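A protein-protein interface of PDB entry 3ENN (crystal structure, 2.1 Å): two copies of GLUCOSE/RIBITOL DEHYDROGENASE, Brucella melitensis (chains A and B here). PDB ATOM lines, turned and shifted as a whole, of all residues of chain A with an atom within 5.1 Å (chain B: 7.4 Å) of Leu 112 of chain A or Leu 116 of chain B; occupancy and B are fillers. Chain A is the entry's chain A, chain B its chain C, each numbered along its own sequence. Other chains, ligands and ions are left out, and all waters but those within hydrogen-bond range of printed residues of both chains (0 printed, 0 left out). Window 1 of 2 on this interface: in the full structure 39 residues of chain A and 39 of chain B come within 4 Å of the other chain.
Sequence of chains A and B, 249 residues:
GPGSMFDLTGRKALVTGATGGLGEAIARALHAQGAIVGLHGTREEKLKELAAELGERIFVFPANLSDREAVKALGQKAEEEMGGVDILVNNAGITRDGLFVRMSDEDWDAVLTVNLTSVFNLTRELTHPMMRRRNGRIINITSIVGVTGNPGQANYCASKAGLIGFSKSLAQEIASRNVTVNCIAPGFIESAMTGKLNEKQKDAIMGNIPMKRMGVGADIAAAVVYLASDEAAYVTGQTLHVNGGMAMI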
ATOM      1  N   TRP A 108      26.120   8.031  -4.682  1.00  0.00           N
ATOM      2  CA  TRP A 108      25.581   7.352  -3.516  1.00  0.00           C
ATOM      3  C   TRP A 108      24.828   6.098  -3.930  1.00  0.00           C
ATOM      4  O   TRP A 108      25.166   4.995  -3.496  1.00  0.00           O
ATOM      5  CB  TRP A 108      24.632   8.262  -2.751  1.00  0.00           C
ATOM      6  CG  TRP A 108      23.983   7.541  -1.614  1.00  0.00           C
ATOM      7  CD1 TRP A 108      22.776   6.901  -1.628  1.00  0.00           C
ATOM      8  CD2 TRP A 108      24.524   7.357  -0.299  1.00  0.00           C
ATOM      9  NE1 TRP A 108      22.525   6.345  -0.397  1.00  0.00           N
ATOM     10  CE2 TRP A 108      23.577   6.616   0.442  1.00  0.00           C
ATOM     11  CE3 TRP A 108      25.703   7.772   0.334  1.00  0.00           C
ATOM     12  CZ2 TRP A 108      23.782   6.258   1.780  1.00  0.00           C
ATOM     13  CZ3 TRP A 108      25.904   7.422   1.678  1.00  0.00           C
ATOM     14  CH2 TRP A 108      24.953   6.671   2.379  1.00  0.00           C
ATOM     15  N   ASP A 109      23.805   6.277  -4.764  1.00  0.00           N
ATOM     16  CA  ASP A 109      22.956   5.169  -5.216  1.00  0.00           C
ATOM     17  C   ASP A 109      23.747   4.055  -5.887  1.00  0.00           C
ATOM     18  O   ASP A 109      23.482   2.881  -5.652  1.00  0.00           O
ATOM     19  CB  ASP A 109      21.884   5.652  -6.195  1.00  0.00           C
ATOM     20  CG  ASP A 109      20.859   6.556  -5.557  1.00  0.00           C
ATOM     21  OD1 ASP A 109      20.880   6.745  -4.319  1.00  0.00           O
ATOM     22  OD2 ASP A 109      20.011   7.084  -6.318  1.00  0.00           O
ATOM     23  N   ALA A 110      24.702   4.410  -6.742  1.00  0.00           N
ATOM     24  CA  ALA A 110      25.476   3.378  -7.433  1.00  0.00           C
ATOM     25  C   ALA A 110      26.255   2.496  -6.436  1.00  0.00           C
ATOM     26  O   ALA A 110      26.236   1.277  -6.547  1.00  0.00           O
ATOM     27  CB  ALA A 110      26.408   3.976  -8.502  1.00  0.00           C
ATOM     28  N   VAL A 111      26.942   3.125  -5.483  1.00  0.00           N
ATOM     29  CA  VAL A 111      27.724   2.392  -4.487  1.00  0.00           C
ATOM     30  C   VAL A 111      26.815   1.541  -3.581  1.00  0.00           C
ATOM     31  O   VAL A 111      27.097   0.386  -3.339  1.00  0.00           O
ATOM     32  CB  VAL A 111      28.654   3.326  -3.672  1.00  0.00           C
ATOM     33  CG1 VAL A 111      29.389   2.565  -2.554  1.00  0.00           C
ATOM     34  CG2 VAL A 111      29.683   3.947  -4.597  1.00  0.00           C
ATOM     35  N   LEU A 112      25.713   2.108  -3.119  1.00  0.00           N
ATOM     36  CA  LEU A 112      24.822   1.379  -2.238  1.00  0.00           C
ATOM     37  C   LEU A 112      24.155   0.205  -2.982  1.00  0.00           C
ATOM     38  O   LEU A 112      24.036  -0.888  -2.439  1.00  0.00           O
ATOM     39  CB  LEU A 112      23.800   2.322  -1.593  1.00  0.00           C
ATOM     40  CG  LEU A 112      24.190   2.969  -0.250  1.00  0.00           C
ATOM     41  CD1 LEU A 112      24.303   1.918   0.864  1.00  0.00           C
ATOM     42  CD2 LEU A 112      25.486   3.822  -0.317  1.00  0.00           C
ATOM     43  N   THR A 113      23.770   0.430  -4.238  1.00  0.00           N
ATOM     44  CA  THR A 113      23.139  -0.604  -5.051  1.00  0.00           C
ATOM     45  C   THR A 113      24.050  -1.813  -5.259  1.00  0.00           C
ATOM     46  O   THR A 113      23.665  -2.946  -4.956  1.00  0.00           O
ATOM     47  CB  THR A 113      22.667  -0.031  -6.411  1.00  0.00           C
ATOM     48  OG1 THR A 113      21.635   0.928  -6.170  1.00  0.00           O
ATOM     49  CG2 THR A 113      22.138  -1.130  -7.339  1.00  0.00           C
ATOM     50  N   VAL A 114      25.251  -1.573  -5.763  1.00  0.00           N
ATOM     51  CA  VAL A 114      26.189  -2.647  -6.026  1.00  0.00           C
ATOM     52  C   VAL A 114      26.720  -3.270  -4.738  1.00  0.00           C
ATOM     53  O   VAL A 114      26.715  -4.496  -4.592  1.00  0.00           O
ATOM     54  CB  VAL A 114      27.381  -2.179  -6.942  1.00  0.00           C
ATOM     55  CG1 VAL A 114      28.479  -3.237  -7.014  1.00  0.00           C
ATOM     56  CG2 VAL A 114      26.893  -1.833  -8.337  1.00  0.00           C
ATOM     57  N   ASN A 115      27.163  -2.427  -3.803  1.00  0.00           N
ATOM     58  CA  ASN A 115      27.897  -2.913  -2.640  1.00  0.00           C
ATOM     59  C   ASN A 115      27.028  -3.525  -1.566  1.00  0.00           C
ATOM     60  O   ASN A 115      27.515  -4.318  -0.772  1.00  0.00           O
ATOM     61  CB  ASN A 115      28.713  -1.797  -1.999  1.00  0.00           C
ATOM     62  CG  ASN A 115      29.842  -1.317  -2.872  1.00  0.00           C
ATOM     63  OD1 ASN A 115      30.642  -0.489  -2.437  1.00  0.00           O
ATOM     64  ND2 ASN A 115      29.909  -1.807  -4.109  1.00  0.00           N
ATOM     65  N   LEU A 116      25.764  -3.120  -1.526  1.00  0.00           N
ATOM     66  CA  LEU A 116      24.862  -3.593  -0.510  1.00  0.00           C
ATOM     67  C   LEU A 116      23.637  -4.315  -1.088  1.00  0.00           C
ATOM     68  O   LEU A 116      23.373  -5.448  -0.729  1.00  0.00           O
ATOM     69  CB  LEU A 116      24.452  -2.447   0.427  1.00  0.00           C
ATOM     70  CG  LEU A 116      23.853  -2.846   1.777  1.00  0.00           C
ATOM     71  CD1 LEU A 116      24.653  -3.959   2.461  1.00  0.00           C
ATOM     72  CD2 LEU A 116      23.743  -1.629   2.678  1.00  0.00           C
ATOM     73  N   THR A 117      22.894  -3.655  -1.973  1.00  0.00           N
ATOM     74  CA  THR A 117      21.674  -4.247  -2.508  1.00  0.00           C
ATOM     75  C   THR A 117      21.934  -5.457  -3.405  1.00  0.00           C
ATOM     76  O   THR A 117      21.225  -6.458  -3.305  1.00  0.00           O
ATOM     77  CB  THR A 117      20.774  -3.187  -3.192  1.00  0.00           C
ATOM     78  OG1 THR A 117      20.345  -2.253  -2.196  1.00  0.00           O
ATOM     79  CG2 THR A 117      19.531  -3.826  -3.842  1.00  0.00           C
ATOM     80  N   SER A 118      22.953  -5.397  -4.254  1.00  0.00           N
ATOM     81  CA  SER A 118      23.285  -6.577  -5.061  1.00  0.00           C
ATOM     82  C   SER A 118      23.687  -7.756  -4.171  1.00  0.00           C
ATOM     83  O   SER A 118      23.423  -8.912  -4.505  1.00  0.00           O
ATOM     84  CB  SER A 118      24.344  -6.277  -6.141  1.00  0.00           C
ATOM     85  OG  SER A 118      25.671  -6.511  -5.673  1.00  0.00           O
ATOM     86  N   ASN A 155      29.619   7.149   0.923  1.00  0.00           N
ATOM     87  CA  ASN A 155      28.877   6.081   0.264  1.00  0.00           C
ATOM     88  C   ASN A 155      29.483   4.689   0.454  1.00  0.00           C
ATOM     89  O   ASN A 155      28.782   3.755   0.852  1.00  0.00           O
ATOM     90  CB  ASN A 155      28.643   6.395  -1.223  1.00  0.00           C
ATOM     91  CG  ASN A 155      29.923   6.737  -1.990  1.00  0.00           C
ATOM     92  OD1 ASN A 155      31.029   6.831  -1.435  1.00  0.00           O
ATOM     93  ND2 ASN A 155      29.762   6.946  -3.292  1.00  0.00           N
ATOM     94  N   ALA A 158      29.337   3.654   4.155  1.00  0.00           N
ATOM     95  CA  ALA A 158      27.966   3.266   4.482  1.00  0.00           C
ATOM     96  C   ALA A 158      27.626   1.860   3.967  1.00  0.00           C
ATOM     97  O   ALA A 158      26.963   1.064   4.648  1.00  0.00           O
ATOM     98  CB  ALA A 158      26.978   4.265   3.921  1.00  0.00           C
ATOM     99  N   SER A 159      28.068   1.569   2.749  1.00  0.00           N
ATOM    100  CA  SER A 159      27.752   0.286   2.137  1.00  0.00           C
ATOM    101  C   SER A 159      28.495  -0.857   2.843  1.00  0.00           C
ATOM    102  O   SER A 159      27.928  -1.910   3.103  1.00  0.00           O
ATOM    103  CB  SER A 159      28.060   0.325   0.637  1.00  0.00           C
ATOM    104  OG  SER A 159      29.440   0.188   0.382  1.00  0.00           O
ATOM    105  N   ALA B  92      14.021   9.658  12.009  1.00  0.00           N
ATOM    106  CA  ALA B  92      12.996   8.911  11.301  1.00  0.00           C
ATOM    107  C   ALA B  92      13.649   7.746  10.596  1.00  0.00           C
ATOM    108  O   ALA B  92      14.680   7.887   9.939  1.00  0.00           O
ATOM    109  CB  ALA B  92      12.256   9.800  10.301  1.00  0.00           C
ATOM    110  N   GLY B  93      13.034   6.594  10.766  1.00  0.00           N
ATOM    111  CA  GLY B  93      13.505   5.341  10.227  1.00  0.00           C
ATOM    112  C   GLY B  93      12.257   4.493  10.198  1.00  0.00           C
ATOM    113  O   GLY B  93      11.291   4.791  10.899  1.00  0.00           O
ATOM    114  N   TRP B 108      13.415  -4.597   1.420  1.00  0.00           N
ATOM    115  CA  TRP B 108      14.807  -4.192   1.477  1.00  0.00           C
ATOM    116  C   TRP B 108      14.979  -2.758   1.019  1.00  0.00           C
ATOM    117  O   TRP B 108      15.524  -1.933   1.744  1.00  0.00           O
ATOM    118  CB  TRP B 108      15.665  -5.129   0.629  1.00  0.00           C
ATOM    119  CG  TRP B 108      17.076  -4.678   0.504  1.00  0.00           C
ATOM    120  CD1 TRP B 108      17.612  -3.920  -0.508  1.00  0.00           C
ATOM    121  CD2 TRP B 108      18.146  -4.953   1.410  1.00  0.00           C
ATOM    122  NE1 TRP B 108      18.947  -3.708  -0.284  1.00  0.00           N
ATOM    123  CE2 TRP B 108      19.306  -4.328   0.885  1.00  0.00           C
ATOM    124  CE3 TRP B 108      18.246  -5.672   2.611  1.00  0.00           C
ATOM    125  CZ2 TRP B 108      20.554  -4.393   1.527  1.00  0.00           C
ATOM    126  CZ3 TRP B 108      19.494  -5.744   3.244  1.00  0.00           C
ATOM    127  CH2 TRP B 108      20.624  -5.106   2.697  1.00  0.00           C
ATOM    128  N   ALA B 110      12.850  -0.297   0.582  1.00  0.00           N
ATOM    129  CA  ALA B 110      12.135   0.697   1.368  1.00  0.00           C
ATOM    130  C   ALA B 110      12.916   1.073   2.618  1.00  0.00           C
ATOM    131  O   ALA B 110      13.047   2.249   2.944  1.00  0.00           O
ATOM    132  CB  ALA B 110      10.754   0.188   1.742  1.00  0.00           C
ATOM    133  N   VAL B 111      13.438   0.070   3.318  1.00  0.00           N
ATOM    134  CA  VAL B 111      14.203   0.327   4.539  1.00  0.00           C
ATOM    135  C   VAL B 111      15.528   1.021   4.206  1.00  0.00           C
ATOM    136  O   VAL B 111      15.891   1.995   4.853  1.00  0.00           O
ATOM    137  CB  VAL B 111      14.411  -0.974   5.353  1.00  0.00           C
ATOM    138  CG1 VAL B 111      15.465  -0.782   6.452  1.00  0.00           C
ATOM    139  CG2 VAL B 111      13.083  -1.400   5.941  1.00  0.00           C
ATOM    140  N   LEU B 112      16.230   0.542   3.188  1.00  0.00           N
ATOM    141  CA  LEU B 112      17.498   1.166   2.815  1.00  0.00           C
ATOM    142  C   LEU B 112      17.328   2.607   2.355  1.00  0.00           C
ATOM    143  O   LEU B 112      18.110   3.478   2.733  1.00  0.00           O
ATOM    144  CB  LEU B 112      18.294   0.323   1.802  1.00  0.00           C
ATOM    145  CG  LEU B 112      19.278  -0.694   2.412  1.00  0.00           C
ATOM    146  CD1 LEU B 112      20.351  -0.008   3.257  1.00  0.00           C
ATOM    147  CD2 LEU B 112      18.543  -1.729   3.273  1.00  0.00           C
ATOM    148  N   THR B 113      16.277   2.857   1.583  1.00  0.00           N
ATOM    149  CA  THR B 113      15.985   4.194   1.053  1.00  0.00           C
ATOM    150  C   THR B 113      15.642   5.195   2.159  1.00  0.00           C
ATOM    151  O   THR B 113      16.211   6.276   2.208  1.00  0.00           O
ATOM    152  CB  THR B 113      14.861   4.130   0.000  1.00  0.00           C
ATOM    153  OG1 THR B 113      15.262   3.222  -1.023  1.00  0.00           O
ATOM    154  CG2 THR B 113      14.598   5.498  -0.635  1.00  0.00           C
ATOM    155  N   VAL B 114      14.732   4.820   3.048  1.00  0.00           N
ATOM    156  CA  VAL B 114      14.311   5.705   4.127  1.00  0.00           C
ATOM    157  C   VAL B 114      15.394   5.824   5.210  1.00  0.00           C
ATOM    158  O   VAL B 114      15.735   6.936   5.646  1.00  0.00           O
ATOM    159  CB  VAL B 114      12.955   5.244   4.714  1.00  0.00           C
ATOM    160  CG1 VAL B 114      12.564   6.051   5.963  1.00  0.00           C
ATOM    161  CG2 VAL B 114      11.871   5.344   3.646  1.00  0.00           C
ATOM    162  N   ASN B 115      15.957   4.686   5.619  1.00  0.00           N
ATOM    163  CA  ASN B 115      16.880   4.673   6.755  1.00  0.00           C
ATOM    164  C   ASN B 115      18.286   5.153   6.439  1.00  0.00           C
ATOM    165  O   ASN B 115      18.993   5.616   7.327  1.00  0.00           O
ATOM    166  CB  ASN B 115      16.943   3.293   7.403  1.00  0.00           C
ATOM    167  CG  ASN B 115      15.653   2.914   8.083  1.00  0.00           C
ATOM    168  OD1 ASN B 115      15.598   1.945   8.843  1.00  0.00           O
ATOM    169  ND2 ASN B 115      14.607   3.681   7.825  1.00  0.00           N
ATOM    170  N   LEU B 116      18.693   5.037   5.184  1.00  0.00           N
ATOM    171  CA  LEU B 116      20.044   5.423   4.822  1.00  0.00           C
ATOM    172  C   LEU B 116      20.057   6.522   3.758  1.00  0.00           C
ATOM    173  O   LEU B 116      20.654   7.574   3.957  1.00  0.00           O
ATOM    174  CB  LEU B 116      20.861   4.201   4.378  1.00  0.00           C
ATOM    175  CG  LEU B 116      22.388   4.240   4.455  1.00  0.00           C
ATOM    176  CD1 LEU B 116      22.890   4.886   5.733  1.00  0.00           C
ATOM    177  CD2 LEU B 116      22.948   2.817   4.300  1.00  0.00           C
ATOM    178  N   THR B 117      19.375   6.286   2.644  1.00  0.00           N
ATOM    179  CA  THR B 117      19.470   7.204   1.521  1.00  0.00           C
ATOM    180  C   THR B 117      18.829   8.548   1.847  1.00  0.00           C
ATOM    181  O   THR B 117      19.392   9.578   1.532  1.00  0.00           O
ATOM    182  CB  THR B 117      18.903   6.574   0.244  1.00  0.00           C
ATOM    183  OG1 THR B 117      19.669   5.400  -0.043  1.00  0.00           O
ATOM    184  CG2 THR B 117      18.976   7.542  -0.945  1.00  0.00           C
ATOM    185  N   SER B 118      17.667   8.538   2.494  1.00  0.00           N
ATOM    186  CA  SER B 118      17.010   9.801   2.815  1.00  0.00           C
ATOM    187  C   SER B 118      17.863  10.581   3.826  1.00  0.00           C
ATOM    188  O   SER B 118      17.954  11.813   3.762  1.00  0.00           O
ATOM    189  CB  SER B 118      15.571   9.577   3.307  1.00  0.00           C
ATOM    190  OG  SER B 118      15.531   9.448   4.710  1.00  0.00           O
ATOM    191  N   VAL B 119      18.514   9.851   4.735  1.00  0.00           N
ATOM    192  CA  VAL B 119      19.508  10.434   5.629  1.00  0.00           C
ATOM    193  C   VAL B 119      20.697  11.039   4.861  1.00  0.00           C
ATOM    194  O   VAL B 119      21.116  12.160   5.147  1.00  0.00           O
ATOM    195  CB  VAL B 119      19.996   9.417   6.676  1.00  0.00           C
ATOM    196  CG1 VAL B 119      21.235   9.954   7.424  1.00  0.00           C
ATOM    197  CG2 VAL B 119      18.868   9.098   7.636  1.00  0.00           C
ATOM    198  N   PHE B 120      21.239  10.295   3.900  1.00  0.00           N
ATOM    199  CA  PHE B 120      22.286  10.825   3.054  1.00  0.00           C
ATOM    200  C   PHE B 120      21.844  12.148   2.393  1.00  0.00           C
ATOM    201  O   PHE B 120      22.581  13.117   2.411  1.00  0.00           O
ATOM    202  CB  PHE B 120      22.711   9.804   1.993  1.00  0.00           C
ATOM    203  CG  PHE B 120      23.338  10.425   0.767  1.00  0.00           C
ATOM    204  CD1 PHE B 120      24.680  10.792   0.764  1.00  0.00           C
ATOM    205  CD2 PHE B 120      22.573  10.654  -0.380  1.00  0.00           C
ATOM    206  CE1 PHE B 120      25.250  11.379  -0.353  1.00  0.00           C
ATOM    207  CE2 PHE B 120      23.132  11.247  -1.507  1.00  0.00           C
ATOM    208  CZ  PHE B 120      24.466  11.600  -1.497  1.00  0.00           C
ATOM    209  N   ASN B 121      20.649  12.180   1.809  1.00  0.00           N
ATOM    210  CA  ASN B 121      20.170  13.413   1.155  1.00  0.00           C
ATOM    211  C   ASN B 121      19.851  14.554   2.114  1.00  0.00           C
ATOM    212  O   ASN B 121      20.231  15.689   1.858  1.00  0.00           O
ATOM    213  CB  ASN B 121      18.987  13.128   0.245  1.00  0.00           C
ATOM    214  CG  ASN B 121      19.419  12.577  -1.089  1.00  0.00           C
ATOM    215  OD1 ASN B 121      19.949  13.305  -1.934  1.00  0.00           O
ATOM    216  ND2 ASN B 121      19.212  11.295  -1.285  1.00  0.00           N
ATOM    217  N   LEU B 122      19.171  14.257   3.214  1.00  0.00           N
ATOM    218  CA  LEU B 122      18.855  15.294   4.195  1.00  0.00           C
ATOM    219  C   LEU B 122      20.148  15.872   4.733  1.00  0.00           C
ATOM    220  O   LEU B 122      20.329  17.095   4.786  1.00  0.00           O
ATOM    221  CB  LEU B 122      18.008  14.746   5.338  1.00  0.00           C
ATOM    222  CG  LEU B 122      16.925  15.629   5.966  1.00  0.00           C
ATOM    223  CD1 LEU B 122      16.783  15.296   7.418  1.00  0.00           C
ATOM    224  CD2 LEU B 122      17.150  17.139   5.791  1.00  0.00           C
ATOM    225  N   THR B 123      21.067  14.981   5.085  1.00  0.00           N
ATOM    226  CA  THR B 123      22.371  15.377   5.596  1.00  0.00           C
ATOM    227  C   THR B 123      23.143  16.213   4.571  1.00  0.00           C
ATOM    228  O   THR B 123      23.730  17.226   4.914  1.00  0.00           O
ATOM    229  CB  THR B 123      23.167  14.151   6.056  1.00  0.00           C
ATOM    230  OG1 THR B 123      22.430  13.468   7.089  1.00  0.00           O
ATOM    231  CG2 THR B 123      24.529  14.560   6.598  1.00  0.00           C
ATOM    232  N   ALA B 158      21.256  -3.646   8.254  1.00  0.00           N
ATOM    233  CA  ALA B 158      22.109  -3.115   7.186  1.00  0.00           C
ATOM    234  C   ALA B 158      22.007  -1.586   7.151  1.00  0.00           C
ATOM    235  O   ALA B 158      23.010  -0.898   7.143  1.00  0.00           O
ATOM    236  CB  ALA B 158      21.726  -3.710   5.843  1.00  0.00           C
ATOM    237  N   SER B 159      20.778  -1.077   7.157  1.00  0.00           N
ATOM    238  CA  SER B 159      20.544   0.353   7.179  1.00  0.00           C
ATOM    239  C   SER B 159      21.176   1.035   8.407  1.00  0.00           C
ATOM    240  O   SER B 159      21.826   2.060   8.275  1.00  0.00           O
ATOM    241  CB  SER B 159      19.040   0.660   7.061  1.00  0.00           C
ATOM    242  OG  SER B 159      18.382   0.619   8.325  1.00  0.00           O
ATOM    243  N   LYS B 160      21.013   0.447   9.583  1.00  0.00           N
ATOM    244  CA  LYS B 160      21.464   1.081  10.816  1.00  0.00           C
ATOM    245  C   LYS B 160      22.978   0.991  11.027  1.00  0.00           C
ATOM    246  O   LYS B 160      23.597   1.932  11.533  1.00  0.00           O
ATOM    247  CB  LYS B 160      20.690   0.540  12.026  1.00  0.00           C
ATOM    248  CG  LYS B 160      19.232   1.008  12.076  1.00  0.00           C
ATOM    249  CD  LYS B 160      19.123   2.517  11.858  1.00  0.00           C
ATOM    250  CE  LYS B 160      17.739   3.015  12.196  1.00  0.00           C
ATOM    251  NZ  LYS B 160      17.691   4.490  12.172  1.00  0.00           N
ATOM    252  N   ALA B 161      23.555  -0.142  10.637  1.00  0.00           N
ATOM    253  CA  ALA B 161      24.995  -0.307  10.579  1.00  0.00           C
ATOM    254  C   ALA B 161      25.628   0.610   9.534  1.00  0.00           C
ATOM    255  O   ALA B 161      26.700   1.177   9.779  1.00  0.00           O
ATOM    256  CB  ALA B 161      25.347  -1.746  10.282  1.00  0.00           C
ATOM    257  N   GLY B 162      24.974   0.720   8.373  1.00  0.00           N
ATOM    258  CA  GLY B 162      25.430   1.602   7.293  1.00  0.00           C
ATOM    259  C   GLY B 162      25.355   3.063   7.675  1.00  0.00           C
ATOM    260  O   GLY B 162      26.230   3.852   7.322  1.00  0.00           O
ATOM    261  N   LEU B 163      24.310   3.419   8.414  1.00  0.00           N
ATOM    262  CA  LEU B 163      24.191   4.747   9.008  1.00  0.00           C
ATOM    263  C   LEU B 163      25.422   5.148   9.841  1.00  0.00           C
ATOM    264  O   LEU B 163      25.931   6.256   9.709  1.00  0.00           O
ATOM    265  CB  LEU B 163      22.926   4.825   9.845  1.00  0.00           C
ATOM    266  CG  LEU B 163      22.620   6.158  10.532  1.00  0.00           C
ATOM    267  CD1 LEU B 163      22.510   7.296   9.518  1.00  0.00           C
ATOM    268  CD2 LEU B 163      21.360   6.016  11.344  1.00  0.00           C
ATOM    269  N   ILE B 164      25.874   4.242  10.698  1.00  0.00           N
ATOM    270  CA  ILE B 164      27.074   4.434  11.489  1.00  0.00           C
ATOM    271  C   ILE B 164      28.316   4.614  10.617  1.00  0.00           C
ATOM    272  O   ILE B 164      29.104   5.508  10.880  1.00  0.00           O
ATOM    273  CB  ILE B 164      27.319   3.234  12.442  1.00  0.00           C
ATOM    274  CG1 ILE B 164      26.188   3.109  13.468  1.00  0.00           C
ATOM    275  CG2 ILE B 164      28.706   3.328  13.089  1.00  0.00           C
ATOM    276  CD1 ILE B 164      26.165   1.782  14.224  1.00  0.00           C
ATOM    277  N   GLY B 165      28.491   3.755   9.613  1.00  0.00           N
ATOM    278  CA  GLY B 165      29.649   3.837   8.717  1.00  0.00           C
ATOM    279  C   GLY B 165      29.671   5.123   7.915  1.00  0.00           C
ATOM    280  O   GLY B 165      30.726   5.743   7.753  1.00  0.00           O
ATOM    281  N   PHE B 166      28.503   5.498   7.396  1.00  0.00           N
ATOM    282  CA  PHE B 166      28.286   6.806   6.803  1.00  0.00           C
ATOM    283  C   PHE B 166      28.716   7.909   7.772  1.00  0.00           C
ATOM    284  O   PHE B 166      29.500   8.790   7.412  1.00  0.00           O
ATOM    285  CB  PHE B 166      26.808   6.969   6.415  1.00  0.00           C
ATOM    286  CG  PHE B 166      26.434   8.377   6.049  1.00  0.00           C
ATOM    287  CD1 PHE B 166      26.845   8.920   4.836  1.00  0.00           C
ATOM    288  CD2 PHE B 166      25.679   9.165   6.927  1.00  0.00           C
ATOM    289  CE1 PHE B 166      26.518  10.232   4.483  1.00  0.00           C
ATOM    290  CE2 PHE B 166      25.346  10.471   6.581  1.00  0.00           C
ATOM    291  CZ  PHE B 166      25.767  10.995   5.344  1.00  0.00           C
ATOM    292  N   SER B 167      28.206   7.855   9.002  1.00  0.00           N
ATOM    293  CA  SER B 167      28.521   8.879  10.014  1.00  0.00           C
ATOM    294  C   SER B 167      30.014   9.015  10.276  1.00  0.00           C
ATOM    295  O   SER B 167      30.524  10.127  10.400  1.00  0.00           O
ATOM    296  CB  SER B 167      27.794   8.601  11.328  1.00  0.00           C
ATOM    297  OG  SER B 167      26.408   8.554  11.085  1.00  0.00           O
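The indole nitrogen (NE1) of Trp 108 of chain A is in hydrogen-bond range of the side-chain hydroxyl (OG1) of Thr 117 of chain B.
The side-chain hydroxyl (OG1) of Thr 117 of chain A is in hydrogen-bond range of the indole nitrogen (NE1) of Trp 108 of chain B (2.8 Å).
O of Leu 112 of chain B is in hydrogen-bond range of N of Thr 117 of chain B (3.1 Å).
OG1 of Thr 113 of chain A is in hydrogen-bond range of O of Asp 109 of chain A (2.7 Å).
The side-chain amide nitrogen of Asn 121 of chain B is in hydrogen-bond range of the backbone carbonyl oxygen of Thr 117 of chain B, at 3.3 Å.
The backbone carbonyl oxygen (O) of Leu 112 of chain A lies within hydrogen-bond range of the backbone NH (N) of Thr 117 of chain A, 3.0 Å away.
Among the printed residues, merely in contact across the chains: Trp 108 of chain A with Leu 116 of chain B, Trp 108 of chain A with Phe 120 of chain B, Trp 108 of chain A with Phe 166 of chain B, Asp 109 of chain A with Thr 117 of chain B, Leu 112 of chain A with Leu 116 of chain B, Leu 116 of chain A with Trp 108 of chain B, Leu 116 of chain A with Leu 112 of chain B, Ala 158 of chain A with Gly 162 of chain B and Ala 158 of chain A with Phe 166 of chain B.
Of chain B, only Leu 116 (3.8 Å) comes within 4 Å of Leu 112 of chain A.
Of chain A, only Trp 108 and Leu 112 come within 4 Å of Leu 116 of chain B.
Of the printed residues of chain A, Phe 166 of chain B touches Trp 108 (3.6 Å) and Ala 158 (3.7 Å).
Printed residues of chain B within 4 Å of Leu 116 of chain A: Trp 108 (3.7 Å) and Leu 112 (3.8 Å).
Ser 159 of chain A touches none of the printed residues of chain B.
Leu 122 of chain B touches none of the printed residues of chain A.
Hydrophobic or aromatic side chains of chain B within 4 Å of the printed part of chain A: Trp 108, Leu 112, Leu 116, Phe 120 and Phe 166.
Along chain B the printed residues that touch a printed residue of chain A span positions 108 to 166.
Among the printed residues, 11 pairs touch across the chains.
Among the printed residues, no Asp or Glu carboxylate lies within 4 Å of a Lys or Arg side-chain nitrogen of the other chain.
Trp 108 of chain A touches Leu 116 of chain B, and with the chains exchanged Leu 116 of chain A touches Trp 108 of chain B.
Trp 108 of chain A touches Thr 117 of chain B, and with the chains exchanged Thr 117 of chain A touches Trp 108 of chain B.
Leu 112 of chain A touches Leu 116 of chain B, and with the chains exchanged Leu 116 of chain A touches Leu 112 of chain B.
12 positions are printed for both chains.
Of the 11 pairs that touch across the chains among the printed residues, 6 have their exchanged pair printed and touching as well.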
